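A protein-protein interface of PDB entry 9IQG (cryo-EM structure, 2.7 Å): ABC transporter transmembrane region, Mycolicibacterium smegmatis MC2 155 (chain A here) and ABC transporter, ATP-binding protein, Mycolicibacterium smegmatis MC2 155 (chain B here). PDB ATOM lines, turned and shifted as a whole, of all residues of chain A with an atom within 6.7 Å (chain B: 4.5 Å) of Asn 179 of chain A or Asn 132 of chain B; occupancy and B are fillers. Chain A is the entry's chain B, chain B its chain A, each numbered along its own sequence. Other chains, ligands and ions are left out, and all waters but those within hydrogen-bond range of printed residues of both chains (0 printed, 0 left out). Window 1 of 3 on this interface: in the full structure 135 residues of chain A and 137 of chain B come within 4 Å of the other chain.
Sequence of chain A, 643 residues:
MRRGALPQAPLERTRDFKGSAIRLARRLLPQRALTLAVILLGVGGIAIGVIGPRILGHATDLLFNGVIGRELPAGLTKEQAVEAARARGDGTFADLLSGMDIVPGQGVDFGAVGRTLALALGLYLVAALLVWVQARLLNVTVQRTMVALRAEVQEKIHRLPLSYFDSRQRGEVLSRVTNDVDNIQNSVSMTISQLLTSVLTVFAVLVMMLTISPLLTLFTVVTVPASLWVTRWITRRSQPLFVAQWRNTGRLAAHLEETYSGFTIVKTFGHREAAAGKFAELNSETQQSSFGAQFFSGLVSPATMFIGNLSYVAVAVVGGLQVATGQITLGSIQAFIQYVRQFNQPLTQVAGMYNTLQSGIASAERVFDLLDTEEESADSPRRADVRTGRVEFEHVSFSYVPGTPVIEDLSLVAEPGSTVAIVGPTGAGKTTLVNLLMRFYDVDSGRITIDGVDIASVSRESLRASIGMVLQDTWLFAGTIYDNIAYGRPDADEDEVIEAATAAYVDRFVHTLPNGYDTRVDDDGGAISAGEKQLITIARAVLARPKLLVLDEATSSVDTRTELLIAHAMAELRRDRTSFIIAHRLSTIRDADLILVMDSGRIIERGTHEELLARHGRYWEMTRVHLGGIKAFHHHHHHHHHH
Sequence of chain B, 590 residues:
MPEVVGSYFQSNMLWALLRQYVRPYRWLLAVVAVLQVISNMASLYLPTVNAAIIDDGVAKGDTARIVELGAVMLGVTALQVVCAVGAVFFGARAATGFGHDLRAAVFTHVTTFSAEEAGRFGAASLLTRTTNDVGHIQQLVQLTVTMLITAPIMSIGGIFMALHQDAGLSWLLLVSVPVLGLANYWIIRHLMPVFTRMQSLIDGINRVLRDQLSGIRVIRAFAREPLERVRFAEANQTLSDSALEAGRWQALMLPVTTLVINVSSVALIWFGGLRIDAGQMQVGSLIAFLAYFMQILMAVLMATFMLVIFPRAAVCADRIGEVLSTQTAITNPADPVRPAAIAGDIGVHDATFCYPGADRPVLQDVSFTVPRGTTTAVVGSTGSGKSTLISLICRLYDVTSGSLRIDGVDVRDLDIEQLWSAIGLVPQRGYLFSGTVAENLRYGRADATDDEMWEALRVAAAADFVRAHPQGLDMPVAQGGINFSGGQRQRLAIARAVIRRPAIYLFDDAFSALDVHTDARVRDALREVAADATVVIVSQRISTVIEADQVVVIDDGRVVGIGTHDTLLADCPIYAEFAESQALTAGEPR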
ATOM      1  N   GLY A 171       5.348 -34.339 -30.726  1.00  0.00           N
ATOM      2  CA  GLY A 171       5.635 -32.961 -30.365  1.00  0.00           C
ATOM      3  C   GLY A 171       6.032 -32.804 -28.911  1.00  0.00           C
ATOM      4  O   GLY A 171       6.885 -31.979 -28.579  1.00  0.00           O
ATOM      5  N   LEU A 174       9.569 -33.971 -28.645  1.00  0.00           N
ATOM      6  CA  LEU A 174      10.427 -32.988 -29.296  1.00  0.00           C
ATOM      7  C   LEU A 174      10.629 -31.758 -28.420  1.00  0.00           C
ATOM      8  O   LEU A 174      11.745 -31.237 -28.316  1.00  0.00           O
ATOM      9  CB  LEU A 174       9.831 -32.600 -30.647  1.00  0.00           C
ATOM     10  CG  LEU A 174      10.640 -31.635 -31.507  1.00  0.00           C
ATOM     11  CD1 LEU A 174      11.980 -32.245 -31.848  1.00  0.00           C
ATOM     12  CD2 LEU A 174       9.876 -31.282 -32.766  1.00  0.00           C
ATOM     13  N   SER A 175       9.558 -31.273 -27.787  1.00  0.00           N
ATOM     14  CA  SER A 175       9.680 -30.128 -26.892  1.00  0.00           C
ATOM     15  C   SER A 175      10.526 -30.468 -25.672  1.00  0.00           C
ATOM     16  O   SER A 175      11.334 -29.648 -25.224  1.00  0.00           O
ATOM     17  CB  SER A 175       8.297 -29.646 -26.461  1.00  0.00           C
ATOM     18  OG  SER A 175       7.593 -30.673 -25.788  1.00  0.00           O
ATOM     19  N   ARG A 176      10.348 -31.667 -25.116  1.00  0.00           N
ATOM     20  CA  ARG A 176      11.176 -32.082 -23.989  1.00  0.00           C
ATOM     21  C   ARG A 176      12.640 -32.223 -24.388  1.00  0.00           C
ATOM     22  O   ARG A 176      13.530 -32.075 -23.543  1.00  0.00           O
ATOM     23  CB  ARG A 176      10.650 -33.398 -23.419  1.00  0.00           C
ATOM     24  CG  ARG A 176      11.285 -33.808 -22.113  1.00  0.00           C
ATOM     25  CD  ARG A 176      10.608 -35.041 -21.555  1.00  0.00           C
ATOM     26  NE  ARG A 176       9.238 -34.761 -21.144  1.00  0.00           N
ATOM     27  CZ  ARG A 176       8.738 -35.067 -19.957  1.00  0.00           C
ATOM     28  NH1 ARG A 176       9.466 -35.680 -19.039  1.00  0.00           N
ATOM     29  NH2 ARG A 176       7.475 -34.756 -19.685  1.00  0.00           N
ATOM     30  N   VAL A 177      12.906 -32.500 -25.659  1.00  0.00           N
ATOM     31  CA  VAL A 177      14.271 -32.725 -26.117  1.00  0.00           C
ATOM     32  C   VAL A 177      14.934 -31.442 -26.613  1.00  0.00           C
ATOM     33  O   VAL A 177      16.128 -31.234 -26.378  1.00  0.00           O
ATOM     34  CB  VAL A 177      14.267 -33.813 -27.203  1.00  0.00           C
ATOM     35  CG1 VAL A 177      15.471 -33.680 -28.113  1.00  0.00           C
ATOM     36  CG2 VAL A 177      14.222 -35.187 -26.564  1.00  0.00           C
ATOM     37  N   THR A 178      14.190 -30.571 -27.289  1.00  0.00           N
ATOM     38  CA  THR A 178      14.738 -29.344 -27.850  1.00  0.00           C
ATOM     39  C   THR A 178      14.404 -28.112 -27.024  1.00  0.00           C
ATOM     40  O   THR A 178      15.305 -27.362 -26.643  1.00  0.00           O
ATOM     41  CB  THR A 178      14.231 -29.146 -29.287  1.00  0.00           C
ATOM     42  OG1 THR A 178      12.809 -28.982 -29.276  1.00  0.00           O
ATOM     43  CG2 THR A 178      14.589 -30.338 -30.151  1.00  0.00           C
ATOM     44  N   ASN A 179      13.121 -27.881 -26.742  1.00  0.00           N
ATOM     45  CA  ASN A 179      12.711 -26.650 -26.076  1.00  0.00           C
ATOM     46  C   ASN A 179      13.212 -26.589 -24.638  1.00  0.00           C
ATOM     47  O   ASN A 179      13.655 -25.533 -24.175  1.00  0.00           O
ATOM     48  CB  ASN A 179      11.190 -26.524 -26.117  1.00  0.00           C
ATOM     49  CG  ASN A 179      10.677 -26.148 -27.489  1.00  0.00           C
ATOM     50  OD1 ASN A 179      11.406 -25.589 -28.305  1.00  0.00           O
ATOM     51  ND2 ASN A 179       9.420 -26.476 -27.758  1.00  0.00           N
ATOM     52  N   ASP A 180      13.140 -27.706 -23.911  1.00  0.00           N
ATOM     53  CA  ASP A 180      13.526 -27.695 -22.504  1.00  0.00           C
ATOM     54  C   ASP A 180      15.021 -27.459 -22.334  1.00  0.00           C
ATOM     55  O   ASP A 180      15.441 -26.762 -21.405  1.00  0.00           O
ATOM     56  CB  ASP A 180      13.107 -29.000 -21.836  1.00  0.00           C
ATOM     57  CG  ASP A 180      11.625 -29.050 -21.547  1.00  0.00           C
ATOM     58  OD1 ASP A 180      10.962 -28.000 -21.657  1.00  0.00           O
ATOM     59  OD2 ASP A 180      11.123 -30.138 -21.204  1.00  0.00           O
ATOM     60  N   VAL A 181      15.840 -28.035 -23.216  1.00  0.00           N
ATOM     61  CA  VAL A 181      17.281 -27.817 -23.142  1.00  0.00           C
ATOM     62  C   VAL A 181      17.619 -26.356 -23.419  1.00  0.00           C
ATOM     63  O   VAL A 181      18.465 -25.759 -22.741  1.00  0.00           O
ATOM     64  CB  VAL A 181      18.008 -28.768 -24.107  1.00  0.00           C
ATOM     65  CG1 VAL A 181      19.507 -28.555 -24.033  1.00  0.00           C
ATOM     66  CG2 VAL A 181      17.662 -30.207 -23.775  1.00  0.00           C
ATOM     67  N   ASP A 182      16.964 -25.757 -24.414  1.00  0.00           N
ATOM     68  CA  ASP A 182      17.180 -24.342 -24.694  1.00  0.00           C
ATOM     69  C   ASP A 182      16.734 -23.474 -23.526  1.00  0.00           C
ATOM     70  O   ASP A 182      17.379 -22.467 -23.208  1.00  0.00           O
ATOM     71  CB  ASP A 182      16.441 -23.945 -25.971  1.00  0.00           C
ATOM     72  CG  ASP A 182      16.844 -24.788 -27.163  1.00  0.00           C
ATOM     73  OD1 ASP A 182      17.960 -25.350 -27.150  1.00  0.00           O
ATOM     74  OD2 ASP A 182      16.041 -24.896 -28.115  1.00  0.00           O
ATOM     75  N   ASN A 183      15.624 -23.840 -22.884  1.00  0.00           N
ATOM     76  CA  ASN A 183      15.157 -23.098 -21.718  1.00  0.00           C
ATOM     77  C   ASN A 183      16.155 -23.189 -20.572  1.00  0.00           C
ATOM     78  O   ASN A 183      16.408 -22.197 -19.879  1.00  0.00           O
ATOM     79  CB  ASN A 183      13.785 -23.616 -21.289  1.00  0.00           C
ATOM     80  CG  ASN A 183      13.015 -22.614 -20.459  1.00  0.00           C
ATOM     81  OD1 ASN A 183      12.982 -22.701 -19.233  1.00  0.00           O
ATOM     82  ND2 ASN A 183      12.389 -21.652 -21.124  1.00  0.00           N
ATOM     83  N   ILE A 184      16.731 -24.373 -20.355  1.00  0.00           N
ATOM     84  CA  ILE A 184      17.762 -24.525 -19.329  1.00  0.00           C
ATOM     85  C   ILE A 184      18.962 -23.646 -19.653  1.00  0.00           C
ATOM     86  O   ILE A 184      19.506 -22.960 -18.779  1.00  0.00           O
ATOM     87  CB  ILE A 184      18.173 -26.000 -19.188  1.00  0.00           C
ATOM     88  CG1 ILE A 184      17.023 -26.831 -18.626  1.00  0.00           C
ATOM     89  CG2 ILE A 184      19.385 -26.128 -18.290  1.00  0.00           C
ATOM     90  CD1 ILE A 184      17.133 -28.297 -18.948  1.00  0.00           C
ATOM     91  N   SER A 363      12.079 -27.030 -16.511  1.00  0.00           N
ATOM     92  CA  SER A 363      12.667 -27.634 -17.702  1.00  0.00           C
ATOM     93  C   SER A 363      13.701 -28.688 -17.332  1.00  0.00           C
ATOM     94  O   SER A 363      13.784 -29.740 -17.976  1.00  0.00           O
ATOM     95  CB  SER A 363      13.289 -26.558 -18.588  1.00  0.00           C
ATOM     96  OG  SER A 363      12.312 -25.644 -19.046  1.00  0.00           O
ATOM     97  N   VAL A 367      13.721 -32.631 -18.369  1.00  0.00           N
ATOM     98  CA  VAL A 367      14.862 -33.234 -19.052  1.00  0.00           C
ATOM     99  C   VAL A 367      15.418 -34.401 -18.246  1.00  0.00           C
ATOM    100  O   VAL A 367      15.755 -35.450 -18.807  1.00  0.00           O
ATOM    101  CB  VAL A 367      15.939 -32.172 -19.336  1.00  0.00           C
ATOM    102  CG1 VAL A 367      17.242 -32.831 -19.758  1.00  0.00           C
ATOM    103  CG2 VAL A 367      15.463 -31.225 -20.411  1.00  0.00           C
ATOM    104  N   THR B 128       5.325 -25.561 -33.361  1.00  0.00           N
ATOM    105  CA  THR B 128       6.389 -24.864 -32.646  1.00  0.00           C
ATOM    106  C   THR B 128       6.215 -23.356 -32.728  1.00  0.00           C
ATOM    107  O   THR B 128       6.380 -22.656 -31.727  1.00  0.00           O
ATOM    108  CB  THR B 128       7.758 -25.270 -33.188  1.00  0.00           C
ATOM    109  OG1 THR B 128       7.779 -25.108 -34.610  1.00  0.00           O
ATOM    110  CG2 THR B 128       8.060 -26.713 -32.836  1.00  0.00           C
ATOM    111  N   THR B 130       3.410 -21.827 -33.260  1.00  0.00           N
ATOM    112  CA  THR B 130       2.172 -21.437 -32.602  1.00  0.00           C
ATOM    113  C   THR B 130       2.316 -21.390 -31.090  1.00  0.00           C
ATOM    114  O   THR B 130       1.576 -20.656 -30.428  1.00  0.00           O
ATOM    115  CB  THR B 130       1.041 -22.401 -32.974  1.00  0.00           C
ATOM    116  OG1 THR B 130       1.065 -22.645 -34.383  1.00  0.00           O
ATOM    117  CG2 THR B 130      -0.310 -21.816 -32.599  1.00  0.00           C
ATOM    118  N   THR B 131       3.253 -22.147 -30.521  1.00  0.00           N
ATOM    119  CA  THR B 131       3.414 -22.157 -29.072  1.00  0.00           C
ATOM    120  C   THR B 131       4.688 -21.465 -28.604  1.00  0.00           C
ATOM    121  O   THR B 131       4.621 -20.456 -27.895  1.00  0.00           O
ATOM    122  CB  THR B 131       3.383 -23.604 -28.560  1.00  0.00           C
ATOM    123  OG1 THR B 131       4.193 -24.431 -29.403  1.00  0.00           O
ATOM    124  CG2 THR B 131       1.966 -24.135 -28.551  1.00  0.00           C
ATOM    125  N   ASN B 132       5.859 -21.947 -29.021  1.00  0.00           N
ATOM    126  CA  ASN B 132       7.103 -21.497 -28.408  1.00  0.00           C
ATOM    127  C   ASN B 132       7.559 -20.144 -28.939  1.00  0.00           C
ATOM    128  O   ASN B 132       8.107 -19.339 -28.182  1.00  0.00           O
ATOM    129  CB  ASN B 132       8.188 -22.550 -28.616  1.00  0.00           C
ATOM    130  CG  ASN B 132       7.827 -23.875 -27.989  1.00  0.00           C
ATOM    131  OD1 ASN B 132       7.513 -24.838 -28.685  1.00  0.00           O
ATOM    132  ND2 ASN B 132       7.856 -23.929 -26.664  1.00  0.00           N
ATOM    133  N   ASP B 133       7.360 -19.875 -30.229  1.00  0.00           N
ATOM    134  CA  ASP B 133       7.707 -18.558 -30.756  1.00  0.00           C
ATOM    135  C   ASP B 133       6.840 -17.473 -30.129  1.00  0.00           C
ATOM    136  O   ASP B 133       7.335 -16.397 -29.760  1.00  0.00           O
ATOM    137  CB  ASP B 133       7.570 -18.551 -32.276  1.00  0.00           C
ATOM    138  CG  ASP B 133       8.442 -19.591 -32.944  1.00  0.00           C
ATOM    139  OD1 ASP B 133       8.938 -20.494 -32.240  1.00  0.00           O
ATOM    140  OD2 ASP B 133       8.641 -19.503 -34.170  1.00  0.00           O
ATOM    141  N   VAL B 134       5.542 -17.748 -29.992  1.00  0.00           N
ATOM    142  CA  VAL B 134       4.654 -16.821 -29.307  1.00  0.00           C
ATOM    143  C   VAL B 134       5.085 -16.649 -27.859  1.00  0.00           C
ATOM    144  O   VAL B 134       5.057 -15.538 -27.320  1.00  0.00           O
ATOM    145  CB  VAL B 134       3.194 -17.301 -29.410  1.00  0.00           C
ATOM    146  CG1 VAL B 134       2.276 -16.341 -28.687  1.00  0.00           C
ATOM    147  CG2 VAL B 134       2.787 -17.436 -30.865  1.00  0.00           C
ATOM    148  N   GLY B 135       5.488 -17.740 -27.207  1.00  0.00           N
ATOM    149  CA  GLY B 135       5.972 -17.631 -25.842  1.00  0.00           C
ATOM    150  C   GLY B 135       7.218 -16.775 -25.730  1.00  0.00           C
ATOM    151  O   GLY B 135       7.381 -16.026 -24.768  1.00  0.00           O
ATOM    152  N   HIS B 136       8.112 -16.874 -26.714  1.00  0.00           N
ATOM    153  CA  HIS B 136       9.320 -16.055 -26.712  1.00  0.00           C
ATOM    154  C   HIS B 136       8.992 -14.576 -26.862  1.00  0.00           C
ATOM    155  O   HIS B 136       9.552 -13.732 -26.149  1.00  0.00           O
ATOM    156  CB  HIS B 136      10.261 -16.508 -27.825  1.00  0.00           C
ATOM    157  CG  HIS B 136      10.918 -17.825 -27.560  1.00  0.00           C
ATOM    158  ND1 HIS B 136      11.564 -18.543 -28.541  1.00  0.00           N
ATOM    159  CD2 HIS B 136      11.029 -18.551 -26.424  1.00  0.00           C
ATOM    160  CE1 HIS B 136      12.044 -19.658 -28.020  1.00  0.00           C
ATOM    161  NE2 HIS B 136      11.733 -19.686 -26.737  1.00  0.00           N
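Of the printed residues of chain A, Asn 132 of chain B touches Asn 179.
Thr 131 of chain B touches none of the printed residues of chain A.
Gly 171 of chain A touches none of the printed residues of chain B.
The nearest printed residue of chain B that does not touch Asn 179 of chain A is Thr 128 of chain B (5.3 Å).
The nearest residue of chain A that does not touch Asn 132 of chain B is Ser 175 of chain A (5.4 Å).
Printed residues of chain B that touch a printed residue of chain A: Asn 132.
Of the 14 printed residues of chain A, 1 touches a printed residue of chain B.
Among the printed residues, no Asp or Glu carboxylate lies within 4 Å of a Lys or Arg side-chain nitrogen of the other chain.
The side-chain amide oxygen (OD1) of Asn 132 of chain B lies within hydrogen-bond range of the side-chain hydroxyl (OG1) of Thr 131 of chain B (3.4 Å).
The side-chain amide nitrogen of Asn 179 of chain A is in hydrogen-bond range of the side-chain amide oxygen of Asn 132 of chain B (2.7 Å).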
